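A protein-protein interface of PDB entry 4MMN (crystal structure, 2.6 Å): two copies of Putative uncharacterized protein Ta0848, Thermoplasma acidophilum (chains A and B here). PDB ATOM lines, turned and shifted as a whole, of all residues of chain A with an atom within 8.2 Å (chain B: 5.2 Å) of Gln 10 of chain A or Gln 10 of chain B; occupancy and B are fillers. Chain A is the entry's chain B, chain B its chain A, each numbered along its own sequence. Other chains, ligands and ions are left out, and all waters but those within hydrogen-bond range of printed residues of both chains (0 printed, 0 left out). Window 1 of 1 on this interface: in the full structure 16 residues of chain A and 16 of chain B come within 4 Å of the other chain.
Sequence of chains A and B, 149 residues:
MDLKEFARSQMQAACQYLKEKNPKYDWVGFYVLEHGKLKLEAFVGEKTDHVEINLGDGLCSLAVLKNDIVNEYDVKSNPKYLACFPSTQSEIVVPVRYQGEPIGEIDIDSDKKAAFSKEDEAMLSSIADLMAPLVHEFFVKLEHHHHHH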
ATOM      1  N   LEU A   3      16.997  13.234 -17.532  1.00  0.00           N
ATOM      2  CA  LEU A   3      17.355  12.122 -16.652  1.00  0.00           C
ATOM      3  C   LEU A   3      17.059  10.836 -17.412  1.00  0.00           C
ATOM      4  O   LEU A   3      17.811   9.863 -17.330  1.00  0.00           O
ATOM      5  CB  LEU A   3      16.580  12.166 -15.337  1.00  0.00           C
ATOM      6  CG  LEU A   3      17.125  13.056 -14.228  1.00  0.00           C
ATOM      7  CD1 LEU A   3      16.274  12.931 -12.976  1.00  0.00           C
ATOM      8  CD2 LEU A   3      18.560  12.658 -13.922  1.00  0.00           C
ATOM      9  N   LYS A   4      15.954  10.848 -18.152  1.00  0.00           N
ATOM     10  CA  LYS A   4      15.550   9.719 -18.973  1.00  0.00           C
ATOM     11  C   LYS A   4      16.682   9.244 -19.867  1.00  0.00           C
ATOM     12  O   LYS A   4      16.939   8.043 -19.971  1.00  0.00           O
ATOM     13  CB  LYS A   4      14.353  10.111 -19.834  1.00  0.00           C
ATOM     14  CG  LYS A   4      13.089  10.341 -19.051  1.00  0.00           C
ATOM     15  CD  LYS A   4      11.888  10.231 -19.959  1.00  0.00           C
ATOM     16  CE  LYS A   4      10.615  10.630 -19.245  1.00  0.00           C
ATOM     17  NZ  LYS A   4       9.443  10.492 -20.154  1.00  0.00           N
ATOM     18  N   GLU A   5      17.351  10.191 -20.514  1.00  0.00           N
ATOM     19  CA  GLU A   5      18.448   9.849 -21.403  1.00  0.00           C
ATOM     20  C   GLU A   5      19.568   9.148 -20.658  1.00  0.00           C
ATOM     21  O   GLU A   5      20.130   8.168 -21.157  1.00  0.00           O
ATOM     22  CB  GLU A   5      18.978  11.085 -22.112  1.00  0.00           C
ATOM     23  CG  GLU A   5      18.172  11.452 -23.341  1.00  0.00           C
ATOM     24  CD  GLU A   5      17.666  10.223 -24.113  1.00  0.00           C
ATOM     25  OE1 GLU A   5      18.499   9.390 -24.554  1.00  0.00           O
ATOM     26  OE2 GLU A   5      16.429  10.094 -24.281  1.00  0.00           O
ATOM     27  N   PHE A   6      19.899   9.656 -19.473  1.00  0.00           N
ATOM     28  CA  PHE A   6      20.910   9.015 -18.631  1.00  0.00           C
ATOM     29  C   PHE A   6      20.483   7.609 -18.243  1.00  0.00           C
ATOM     30  O   PHE A   6      21.264   6.652 -18.298  1.00  0.00           O
ATOM     31  CB  PHE A   6      21.153   9.829 -17.362  1.00  0.00           C
ATOM     32  CG  PHE A   6      21.922   9.090 -16.300  1.00  0.00           C
ATOM     33  CD1 PHE A   6      23.281   8.841 -16.449  1.00  0.00           C
ATOM     34  CD2 PHE A   6      21.287   8.644 -15.147  1.00  0.00           C
ATOM     35  CE1 PHE A   6      23.994   8.156 -15.463  1.00  0.00           C
ATOM     36  CE2 PHE A   6      21.988   7.957 -14.159  1.00  0.00           C
ATOM     37  CZ  PHE A   6      23.340   7.713 -14.315  1.00  0.00           C
ATOM     38  N   ALA A   7      19.228   7.497 -17.833  1.00  0.00           N
ATOM     39  CA  ALA A   7      18.690   6.216 -17.460  1.00  0.00           C
ATOM     40  C   ALA A   7      18.740   5.294 -18.663  1.00  0.00           C
ATOM     41  O   ALA A   7      19.174   4.145 -18.550  1.00  0.00           O
ATOM     42  CB  ALA A   7      17.294   6.364 -16.946  1.00  0.00           C
ATOM     43  N   ARG A   8      18.328   5.810 -19.819  1.00  0.00           N
ATOM     44  CA  ARG A   8      18.363   5.010 -21.023  1.00  0.00           C
ATOM     45  C   ARG A   8      19.782   4.566 -21.263  1.00  0.00           C
ATOM     46  O   ARG A   8      20.034   3.388 -21.529  1.00  0.00           O
ATOM     47  CB  ARG A   8      17.833   5.771 -22.229  1.00  0.00           C
ATOM     48  CG  ARG A   8      17.826   4.904 -23.471  1.00  0.00           C
ATOM     49  CD  ARG A   8      17.145   5.576 -24.649  1.00  0.00           C
ATOM     50  NE  ARG A   8      15.679   5.545 -24.575  1.00  0.00           N
ATOM     51  CZ  ARG A   8      14.924   6.617 -24.355  1.00  0.00           C
ATOM     52  NH1 ARG A   8      15.496   7.797 -24.172  1.00  0.00           N
ATOM     53  NH2 ARG A   8      13.604   6.515 -24.311  1.00  0.00           N
ATOM     54  N   SER A   9      20.705   5.509 -21.107  1.00  0.00           N
ATOM     55  CA  SER A   9      22.127   5.222 -21.219  1.00  0.00           C
ATOM     56  C   SER A   9      22.507   4.004 -20.371  1.00  0.00           C
ATOM     57  O   SER A   9      23.123   3.063 -20.881  1.00  0.00           O
ATOM     58  CB  SER A   9      22.947   6.458 -20.809  1.00  0.00           C
ATOM     59  OG  SER A   9      24.242   6.127 -20.324  1.00  0.00           O
ATOM     60  N   GLN A  10      22.100   3.999 -19.101  1.00  0.00           N
ATOM     61  CA  GLN A  10      22.433   2.898 -18.198  1.00  0.00           C
ATOM     62  C   GLN A  10      21.740   1.612 -18.633  1.00  0.00           C
ATOM     63  O   GLN A  10      22.327   0.528 -18.580  1.00  0.00           O
ATOM     64  CB  GLN A  10      22.066   3.246 -16.761  1.00  0.00           C
ATOM     65  CG  GLN A  10      22.909   4.378 -16.158  1.00  0.00           C
ATOM     66  CD  GLN A  10      24.407   4.078 -16.104  1.00  0.00           C
ATOM     67  OE1 GLN A  10      25.223   4.784 -16.729  1.00  0.00           O
ATOM     68  NE2 GLN A  10      24.782   3.039 -15.338  1.00  0.00           N
ATOM     69  N   MET A  11      20.495   1.737 -19.081  1.00  0.00           N
ATOM     70  CA  MET A  11      19.712   0.568 -19.463  1.00  0.00           C
ATOM     71  C   MET A  11      20.310  -0.108 -20.686  1.00  0.00           C
ATOM     72  O   MET A  11      20.340  -1.340 -20.792  1.00  0.00           O
ATOM     73  CB  MET A  11      18.266   0.969 -19.722  1.00  0.00           C
ATOM     74  CG  MET A  11      17.488   1.243 -18.451  1.00  0.00           C
ATOM     75  SD  MET A  11      15.892   2.015 -18.765  1.00  0.00           S
ATOM     76  CE  MET A  11      14.946   0.615 -19.284  1.00  0.00           C
ATOM     77  N   GLN A  12      20.792   0.708 -21.612  1.00  0.00           N
ATOM     78  CA  GLN A  12      21.449   0.180 -22.791  1.00  0.00           C
ATOM     79  C   GLN A  12      22.724  -0.560 -22.375  1.00  0.00           C
ATOM     80  O   GLN A  12      22.982  -1.685 -22.814  1.00  0.00           O
ATOM     81  CB  GLN A  12      21.767   1.315 -23.762  1.00  0.00           C
ATOM     82  CG  GLN A  12      21.746   0.887 -25.195  1.00  0.00           C
ATOM     83  CD  GLN A  12      20.384   0.365 -25.586  1.00  0.00           C
ATOM     84  OE1 GLN A  12      19.371   1.057 -25.439  1.00  0.00           O
ATOM     85  NE2 GLN A  12      20.347  -0.870 -26.072  1.00  0.00           N
ATOM     86  N   ALA A  13      23.489   0.068 -21.486  1.00  0.00           N
ATOM     87  CA  ALA A  13      24.743  -0.502 -21.013  1.00  0.00           C
ATOM     88  C   ALA A  13      24.506  -1.832 -20.313  1.00  0.00           C
ATOM     89  O   ALA A  13      25.312  -2.768 -20.436  1.00  0.00           O
ATOM     90  CB  ALA A  13      25.445   0.472 -20.074  1.00  0.00           C
ATOM     91  N   ALA A  14      23.389  -1.917 -19.596  1.00  0.00           N
ATOM     92  CA  ALA A  14      23.049  -3.144 -18.904  1.00  0.00           C
ATOM     93  C   ALA A  14      22.752  -4.222 -19.943  1.00  0.00           C
ATOM     94  O   ALA A  14      23.294  -5.330 -19.871  1.00  0.00           O
ATOM     95  CB  ALA A  14      21.874  -2.929 -17.985  1.00  0.00           C
ATOM     96  N   CYS A  15      21.924  -3.878 -20.929  1.00  0.00           N
ATOM     97  CA  CYS A  15      21.631  -4.783 -22.031  1.00  0.00           C
ATOM     98  C   CYS A  15      22.899  -5.292 -22.707  1.00  0.00           C
ATOM     99  O   CYS A  15      23.025  -6.484 -23.031  1.00  0.00           O
ATOM    100  CB  CYS A  15      20.783  -4.083 -23.075  1.00  0.00           C
ATOM    101  SG  CYS A  15      19.088  -3.865 -22.683  1.00  0.00           S
ATOM    102  N   GLN A  16      23.843  -4.377 -22.898  1.00  0.00           N
ATOM    103  CA  GLN A  16      25.092  -4.708 -23.556  1.00  0.00           C
ATOM    104  C   GLN A  16      25.856  -5.710 -22.732  1.00  0.00           C
ATOM    105  O   GLN A  16      26.124  -6.819 -23.204  1.00  0.00           O
ATOM    106  CB  GLN A  16      25.934  -3.460 -23.773  1.00  0.00           C
ATOM    107  CG  GLN A  16      27.064  -3.687 -24.726  1.00  0.00           C
ATOM    108  CD  GLN A  16      26.547  -4.088 -26.086  1.00  0.00           C
ATOM    109  OE1 GLN A  16      25.717  -3.393 -26.686  1.00  0.00           O
ATOM    110  NE2 GLN A  16      27.015  -5.229 -26.576  1.00  0.00           N
ATOM    111  N   TYR A  17      26.157  -5.330 -21.490  1.00  0.00           N
ATOM    112  CA  TYR A  17      26.888  -6.193 -20.571  1.00  0.00           C
ATOM    113  C   TYR A  17      26.244  -7.569 -20.514  1.00  0.00           C
ATOM    114  O   TYR A  17      26.930  -8.589 -20.537  1.00  0.00           O
ATOM    115  CB  TYR A  17      26.936  -5.564 -19.185  1.00  0.00           C
ATOM    116  CG  TYR A  17      27.594  -6.407 -18.114  1.00  0.00           C
ATOM    117  CD1 TYR A  17      26.867  -7.361 -17.411  1.00  0.00           C
ATOM    118  CD2 TYR A  17      28.921  -6.206 -17.752  1.00  0.00           C
ATOM    119  CE1 TYR A  17      27.446  -8.118 -16.419  1.00  0.00           C
ATOM    120  CE2 TYR A  17      29.517  -6.964 -16.746  1.00  0.00           C
ATOM    121  CZ  TYR A  17      28.766  -7.920 -16.090  1.00  0.00           C
ATOM    122  OH  TYR A  17      29.317  -8.692 -15.095  1.00  0.00           O
ATOM    123  N   LEU A  18      24.922  -7.606 -20.470  1.00  0.00           N
ATOM    124  CA  LEU A  18      24.232  -8.891 -20.445  1.00  0.00           C
ATOM    125  C   LEU A  18      24.469  -9.704 -21.718  1.00  0.00           C
ATOM    126  O   LEU A  18      24.839 -10.878 -21.648  1.00  0.00           O
ATOM    127  CB  LEU A  18      22.730  -8.696 -20.208  1.00  0.00           C
ATOM    128  CG  LEU A  18      22.372  -8.407 -18.747  1.00  0.00           C
ATOM    129  CD1 LEU A  18      20.878  -8.320 -18.576  1.00  0.00           C
ATOM    130  CD2 LEU A  18      22.970  -9.458 -17.810  1.00  0.00           C
ATOM    131  N   PHE A  30      14.643  -4.061 -22.243  1.00  0.00           N
ATOM    132  CA  PHE A  30      13.948  -3.529 -21.080  1.00  0.00           C
ATOM    133  C   PHE A  30      12.589  -2.982 -21.445  1.00  0.00           C
ATOM    134  O   PHE A  30      12.521  -1.995 -22.167  1.00  0.00           O
ATOM    135  CB  PHE A  30      14.749  -2.408 -20.447  1.00  0.00           C
ATOM    136  CG  PHE A  30      15.805  -2.851 -19.461  1.00  0.00           C
ATOM    137  CD1 PHE A  30      17.100  -3.144 -19.867  1.00  0.00           C
ATOM    138  CD2 PHE A  30      15.514  -2.906 -18.095  1.00  0.00           C
ATOM    139  CE1 PHE A  30      18.081  -3.522 -18.923  1.00  0.00           C
ATOM    140  CE2 PHE A  30      16.490  -3.287 -17.148  1.00  0.00           C
ATOM    141  CZ  PHE A  30      17.772  -3.588 -17.566  1.00  0.00           C
ATOM    142  N   ALA A  42      14.970   0.234 -24.103  1.00  0.00           N
ATOM    143  CA  ALA A  42      16.378  -0.080 -24.309  1.00  0.00           C
ATOM    144  C   ALA A  42      16.475  -1.540 -24.686  1.00  0.00           C
ATOM    145  O   ALA A  42      15.745  -2.361 -24.152  1.00  0.00           O
ATOM    146  CB  ALA A  42      17.219   0.216 -23.068  1.00  0.00           C
ATOM    147  N   ILE A 127      19.819  -8.171 -10.889  1.00  0.00           N
ATOM    148  CA  ILE A 127      20.091  -7.075 -11.784  1.00  0.00           C
ATOM    149  C   ILE A 127      18.827  -6.223 -11.884  1.00  0.00           C
ATOM    150  O   ILE A 127      18.892  -4.988 -11.896  1.00  0.00           O
ATOM    151  CB  ILE A 127      20.540  -7.590 -13.167  1.00  0.00           C
ATOM    152  CG1 ILE A 127      21.948  -8.182 -13.065  1.00  0.00           C
ATOM    153  CG2 ILE A 127      20.470  -6.490 -14.204  1.00  0.00           C
ATOM    154  CD1 ILE A 127      22.445  -8.765 -14.353  1.00  0.00           C
ATOM    155  N   LEU A 130      18.819  -3.943  -8.857  1.00  0.00           N
ATOM    156  CA  LEU A 130      19.822  -2.877  -8.971  1.00  0.00           C
ATOM    157  C   LEU A 130      19.420  -1.808  -9.993  1.00  0.00           C
ATOM    158  O   LEU A 130      19.761  -0.611  -9.834  1.00  0.00           O
ATOM    159  CB  LEU A 130      21.189  -3.470  -9.344  1.00  0.00           C
ATOM    160  CG  LEU A 130      21.944  -4.306  -8.305  1.00  0.00           C
ATOM    161  CD1 LEU A 130      23.105  -5.056  -8.919  1.00  0.00           C
ATOM    162  CD2 LEU A 130      22.478  -3.357  -7.242  1.00  0.00           C
ATOM    163  N   MET A 131      18.680  -2.234 -11.019  1.00  0.00           N
ATOM    164  CA  MET A 131      18.364  -1.350 -12.126  1.00  0.00           C
ATOM    165  C   MET A 131      17.061  -0.608 -11.905  1.00  0.00           C
ATOM    166  O   MET A 131      16.743   0.336 -12.639  1.00  0.00           O
ATOM    167  CB  MET A 131      18.286  -2.127 -13.435  1.00  0.00           C
ATOM    168  CG  MET A 131      19.605  -2.751 -13.885  1.00  0.00           C
ATOM    169  SD  MET A 131      20.916  -1.522 -14.120  1.00  0.00           S
ATOM    170  CE  MET A 131      20.120  -0.365 -15.219  1.00  0.00           C
ATOM    171  N   LEU A 134      16.576   3.253 -11.992  1.00  0.00           N
ATOM    172  CA  LEU A 134      16.855   3.735 -13.312  1.00  0.00           C
ATOM    173  C   LEU A 134      15.648   3.447 -14.189  1.00  0.00           C
ATOM    174  O   LEU A 134      15.172   4.316 -14.918  1.00  0.00           O
ATOM    175  CB  LEU A 134      18.146   3.117 -13.852  1.00  0.00           C
ATOM    176  CG  LEU A 134      19.367   3.777 -13.178  1.00  0.00           C
ATOM    177  CD1 LEU A 134      20.608   2.895 -13.230  1.00  0.00           C
ATOM    178  CD2 LEU A 134      19.662   5.174 -13.747  1.00  0.00           C
ATOM    179  N   VAL A 135      15.124   2.239 -14.095  1.00  0.00           N
ATOM    180  CA  VAL A 135      13.964   1.904 -14.895  1.00  0.00           C
ATOM    181  C   VAL A 135      12.799   2.852 -14.580  1.00  0.00           C
ATOM    182  O   VAL A 135      12.133   3.372 -15.488  1.00  0.00           O
ATOM    183  CB  VAL A 135      13.533   0.469 -14.654  1.00  0.00           C
ATOM    184  CG1 VAL A 135      12.387   0.126 -15.585  1.00  0.00           C
ATOM    185  CG2 VAL A 135      14.692  -0.457 -14.897  1.00  0.00           C
ATOM    186  N   PHE A 138      11.092   5.979 -16.389  1.00  0.00           N
ATOM    187  CA  PHE A 138      10.197   5.926 -17.539  1.00  0.00           C
ATOM    188  C   PHE A 138       8.800   5.483 -17.150  1.00  0.00           C
ATOM    189  O   PHE A 138       7.912   5.373 -17.992  1.00  0.00           O
ATOM    190  CB  PHE A 138      10.755   4.991 -18.610  1.00  0.00           C
ATOM    191  CG  PHE A 138      11.920   5.559 -19.355  1.00  0.00           C
ATOM    192  CD1 PHE A 138      11.729   6.464 -20.392  1.00  0.00           C
ATOM    193  CD2 PHE A 138      13.212   5.182 -19.029  1.00  0.00           C
ATOM    194  CE1 PHE A 138      12.819   6.987 -21.092  1.00  0.00           C
ATOM    195  CE2 PHE A 138      14.308   5.692 -19.721  1.00  0.00           C
ATOM    196  CZ  PHE A 138      14.113   6.597 -20.756  1.00  0.00           C
ATOM    197  N   PHE B   6      29.415  -6.270 -12.846  1.00  0.00           N
ATOM    198  CA  PHE B   6      28.331  -5.593 -13.547  1.00  0.00           C
ATOM    199  C   PHE B   6      28.144  -4.198 -13.022  1.00  0.00           C
ATOM    200  O   PHE B   6      27.990  -3.249 -13.783  1.00  0.00           O
ATOM    201  CB  PHE B   6      27.011  -6.343 -13.400  1.00  0.00           C
ATOM    202  CG  PHE B   6      25.812  -5.537 -13.840  1.00  0.00           C
ATOM    203  CD1 PHE B   6      25.598  -5.269 -15.183  1.00  0.00           C
ATOM    204  CD2 PHE B   6      24.903  -5.053 -12.918  1.00  0.00           C
ATOM    205  CE1 PHE B   6      24.504  -4.534 -15.605  1.00  0.00           C
ATOM    206  CE2 PHE B   6      23.812  -4.315 -13.333  1.00  0.00           C
ATOM    207  CZ  PHE B   6      23.613  -4.057 -14.684  1.00  0.00           C
ATOM    208  N   ALA B   7      28.160  -4.093 -11.700  1.00  0.00           N
ATOM    209  CA  ALA B   7      27.982  -2.825 -11.028  1.00  0.00           C
ATOM    210  C   ALA B   7      29.059  -1.847 -11.468  1.00  0.00           C
ATOM    211  O   ALA B   7      28.775  -0.667 -11.721  1.00  0.00           O
ATOM    212  CB  ALA B   7      28.010  -3.012  -9.532  1.00  0.00           C
ATOM    213  N   ARG B   8      30.298  -2.320 -11.535  1.00  0.00           N
ATOM    214  CA  ARG B   8      31.373  -1.472 -12.018  1.00  0.00           C
ATOM    215  C   ARG B   8      31.066  -1.047 -13.453  1.00  0.00           C
ATOM    216  O   ARG B   8      31.227   0.121 -13.798  1.00  0.00           O
ATOM    217  CB  ARG B   8      32.724  -2.171 -11.931  1.00  0.00           C
ATOM    218  CG  ARG B   8      33.850  -1.276 -12.382  1.00  0.00           C
ATOM    219  CD  ARG B   8      35.197  -1.896 -12.167  1.00  0.00           C
ATOM    220  NE  ARG B   8      35.584  -1.822 -10.769  1.00  0.00           N
ATOM    221  CZ  ARG B   8      35.666  -2.877  -9.975  1.00  0.00           C
ATOM    222  NH1 ARG B   8      35.385  -4.085 -10.462  1.00  0.00           N
ATOM    223  NH2 ARG B   8      36.037  -2.723  -8.703  1.00  0.00           N
ATOM    224  N   SER B   9      30.605  -1.991 -14.273  1.00  0.00           N
ATOM    225  CA  SER B   9      30.192  -1.670 -15.628  1.00  0.00           C
ATOM    226  C   SER B   9      29.243  -0.471 -15.625  1.00  0.00           C
ATOM    227  O   SER B   9      29.477   0.504 -16.328  1.00  0.00           O
ATOM    228  CB  SER B   9      29.535  -2.886 -16.293  1.00  0.00           C
ATOM    229  OG  SER B   9      28.618  -2.493 -17.308  1.00  0.00           O
ATOM    230  N   GLN B  10      28.216  -0.504 -14.783  1.00  0.00           N
ATOM    231  CA  GLN B  10      27.248   0.588 -14.760  1.00  0.00           C
ATOM    232  C   GLN B  10      27.875   1.894 -14.311  1.00  0.00           C
ATOM    233  O   GLN B  10      27.601   2.954 -14.882  1.00  0.00           O
ATOM    234  CB  GLN B  10      26.076   0.245 -13.837  1.00  0.00           C
ATOM    235  CG  GLN B  10      25.234  -0.877 -14.373  1.00  0.00           C
ATOM    236  CD  GLN B  10      24.660  -0.539 -15.730  1.00  0.00           C
ATOM    237  OE1 GLN B  10      23.894   0.428 -15.875  1.00  0.00           O
ATOM    238  NE2 GLN B  10      25.048  -1.321 -16.749  1.00  0.00           N
ATOM    239  N   MET B  11      28.728   1.808 -13.298  1.00  0.00           N
ATOM    240  CA  MET B  11      29.320   2.997 -12.699  1.00  0.00           C
ATOM    241  C   MET B  11      30.268   3.672 -13.666  1.00  0.00           C
ATOM    242  O   MET B  11      30.309   4.905 -13.774  1.00  0.00           O
ATOM    243  CB  MET B  11      30.050   2.629 -11.416  1.00  0.00           C
ATOM    244  CG  MET B  11      29.120   2.298 -10.279  1.00  0.00           C
ATOM    245  SD  MET B  11      29.993   1.601  -8.862  1.00  0.00           S
ATOM    246  CE  MET B  11      30.661   3.051  -8.093  1.00  0.00           C
ATOM    247  N   GLN B  12      31.022   2.851 -14.387  1.00  0.00           N
ATOM    248  CA  GLN B  12      31.957   3.377 -15.361  1.00  0.00           C
ATOM    249  C   GLN B  12      31.152   4.092 -16.428  1.00  0.00           C
ATOM    250  O   GLN B  12      31.457   5.237 -16.771  1.00  0.00           O
ATOM    251  CB  GLN B  12      32.835   2.262 -15.943  1.00  0.00           C
ATOM    252  CG  GLN B  12      34.244   2.727 -16.356  1.00  0.00           C
ATOM    253  CD  GLN B  12      35.079   3.308 -15.191  1.00  0.00           C
ATOM    254  OE1 GLN B  12      35.307   2.664 -14.153  1.00  0.00           O
ATOM    255  NE2 GLN B  12      35.533   4.544 -15.375  1.00  0.00           N
ATOM    256  N   ALA B  13      30.072   3.455 -16.867  1.00  0.00           N
ATOM    257  CA  ALA B  13      29.226   4.005 -17.906  1.00  0.00           C
ATOM    258  C   ALA B  13      28.643   5.335 -17.476  1.00  0.00           C
ATOM    259  O   ALA B  13      28.446   6.244 -18.284  1.00  0.00           O
ATOM    260  CB  ALA B  13      28.128   3.031 -18.247  1.00  0.00           C
ATOM    261  N   ALA B  14      28.360   5.448 -16.193  1.00  0.00           N
ATOM    262  CA  ALA B  14      27.810   6.683 -15.676  1.00  0.00           C
ATOM    263  C   ALA B  14      28.847   7.801 -15.753  1.00  0.00           C
ATOM    264  O   ALA B  14      28.558   8.906 -16.214  1.00  0.00           O
ATOM    265  CB  ALA B  14      27.343   6.487 -14.263  1.00  0.00           C
ATOM    266  N   CYS B  15      30.056   7.493 -15.295  1.00  0.00           N
ATOM    267  CA  CYS B  15      31.168   8.421 -15.357  1.00  0.00           C
ATOM    268  C   CYS B  15      31.353   8.940 -16.780  1.00  0.00           C
ATOM    269  O   CYS B  15      31.562  10.142 -17.011  1.00  0.00           O
ATOM    270  CB  CYS B  15      32.442   7.731 -14.884  1.00  0.00           C
ATOM    271  SG  CYS B  15      32.555   7.501 -13.098  1.00  0.00           S
ATOM    272  N   MET B 131      21.754   5.701  -8.823  1.00  0.00           N
ATOM    273  CA  MET B 131      22.901   4.796  -8.859  1.00  0.00           C
ATOM    274  C   MET B 131      23.140   4.079  -7.535  1.00  0.00           C
ATOM    275  O   MET B 131      23.911   3.096  -7.463  1.00  0.00           O
ATOM    276  CB  MET B 131      24.158   5.579  -9.263  1.00  0.00           C
ATOM    277  CG  MET B 131      24.066   6.140 -10.671  1.00  0.00           C
ATOM    278  SD  MET B 131      23.927   4.811 -11.892  1.00  0.00           S
ATOM    279  CE  MET B 131      25.420   3.880 -11.530  1.00  0.00           C
ATOM    280  N   LEU B 134      23.401   0.308  -7.112  1.00  0.00           N
ATOM    281  CA  LEU B 134      24.540  -0.214  -7.832  1.00  0.00           C
ATOM    282  C   LEU B 134      25.812   0.018  -7.069  1.00  0.00           C
ATOM    283  O   LEU B 134      26.603  -0.912  -6.881  1.00  0.00           O
ATOM    284  CB  LEU B 134      24.632   0.437  -9.198  1.00  0.00           C
ATOM    285  CG  LEU B 134      23.678  -0.120 -10.236  1.00  0.00           C
ATOM    286  CD1 LEU B 134      23.404   0.923 -11.283  1.00  0.00           C
ATOM    287  CD2 LEU B 134      24.334  -1.336 -10.867  1.00  0.00           C
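The side-chain amide oxygen (OE1) of Gln 10 of chain B is in hydrogen-bond range of the side-chain amide nitrogen (NE2) of Gln 10 of chain A (2.8 Å). The backbone NH (N) of Phe 6 of chain B is in hydrogen-bond range of the side-chain hydroxyl (OH) of Tyr 17 of chain A, at 3.3 Å. The backbone NH of Ala 14 of chain A lies close to the side-chain amide nitrogen of Gln 10 of chain B. N of Ala 14 of chain B lies within hydrogen-bond range of OE1 of Gln 10 of chain A.
Gln 10 of chain A touches four residues of chain B. Of chain A, only Tyr 17 (3.7 Å) comes within 4 Å of Ser 9 of chain B. Of the printed residues of chain B, Tyr 17 of chain A touches Phe 6 (3.3 Å) and Ser 9 (3.7 Å). Of the printed residues of chain B, Leu 134 of chain A touches Leu 134. Printed residues of chain A within 4 Å of Met 131 of chain B: Phe 6 and Gln 10. Printed residues of chain A within 4 Å of Leu 134 of chain B: Leu 130 and Leu 134. The nearest residue of chain B that does not touch Gln 10 of chain A is Met 11 of chain B (4.6 Å). The nearest printed residue of chain B that does not touch Met 131 of chain A is Leu 134 of chain B (4.5 Å).
Of the 12 printed residues of chain B, 7 touch a printed residue of chain A. Printed residues of chain B that touch a printed residue of chain A: Phe 6, Ser 9, Gln 10, Ala 13, Ala 14, Met 131 and Leu 134. Of the 24 printed residues of chain A, 8 touch a printed residue of chain B. Among the printed residues, 15 pairs touch across the chains. Among the printed residues, no Asp or Glu carboxylate lies within 4 Å of a Lys or Arg side-chain nitrogen of the other chain.
Phe 6 of chain A touches Ala 14 of chain B, and with the chains exchanged Ala 14 of chain A touches Phe 6 of chain B. Phe 6 of chain A touches Met 131 of chain B, and with the chains exchanged Met 131 of chain A touches Phe 6 of chain B. Gln 10 of chain A touches Ala 13 of chain B, and with the chains exchanged Ala 13 of chain A touches Gln 10 of chain B. Leu 134 of chain B touches its own counterpart, Leu 134 of chain A. Positions printed for both chains: 6, 7, 8, 9, 10, 11, 12, 13, 14, 15, 131 and 134. Of the 15 pairs that touch across the chains among the printed residues, 12 have their exchanged pair printed and touching as well.
Among the printed residues, pairs that only touch across the chains: Phe 6 of chain A with Ala 14 of chain B (3.9 Å), Phe 6 of chain A with Met 131 of chain B (3.8 Å), Gln 10 of chain A with Ala 13 of chain B (3.5 Å), Gln 10 of chain A with Met 131 of chain B (3.95 Å), Ala 13 of chain A with Gln 10 of chain B (3.6 Å), Ala 14 of chain A with Phe 6 of chain B (3.9 Å), Tyr 17 of chain A with Ser 9 of chain B (3.7 Å), Leu 130 of chain A with Leu 134 of chain B (3.8 Å), Met 131 of chain A with Phe 6 of chain B (3.7 Å), Met 131 of chain A with Gln 10 of chain B (3.9 Å) and Leu 134 of chain A with Leu 134 of chain B (3.9 Å).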
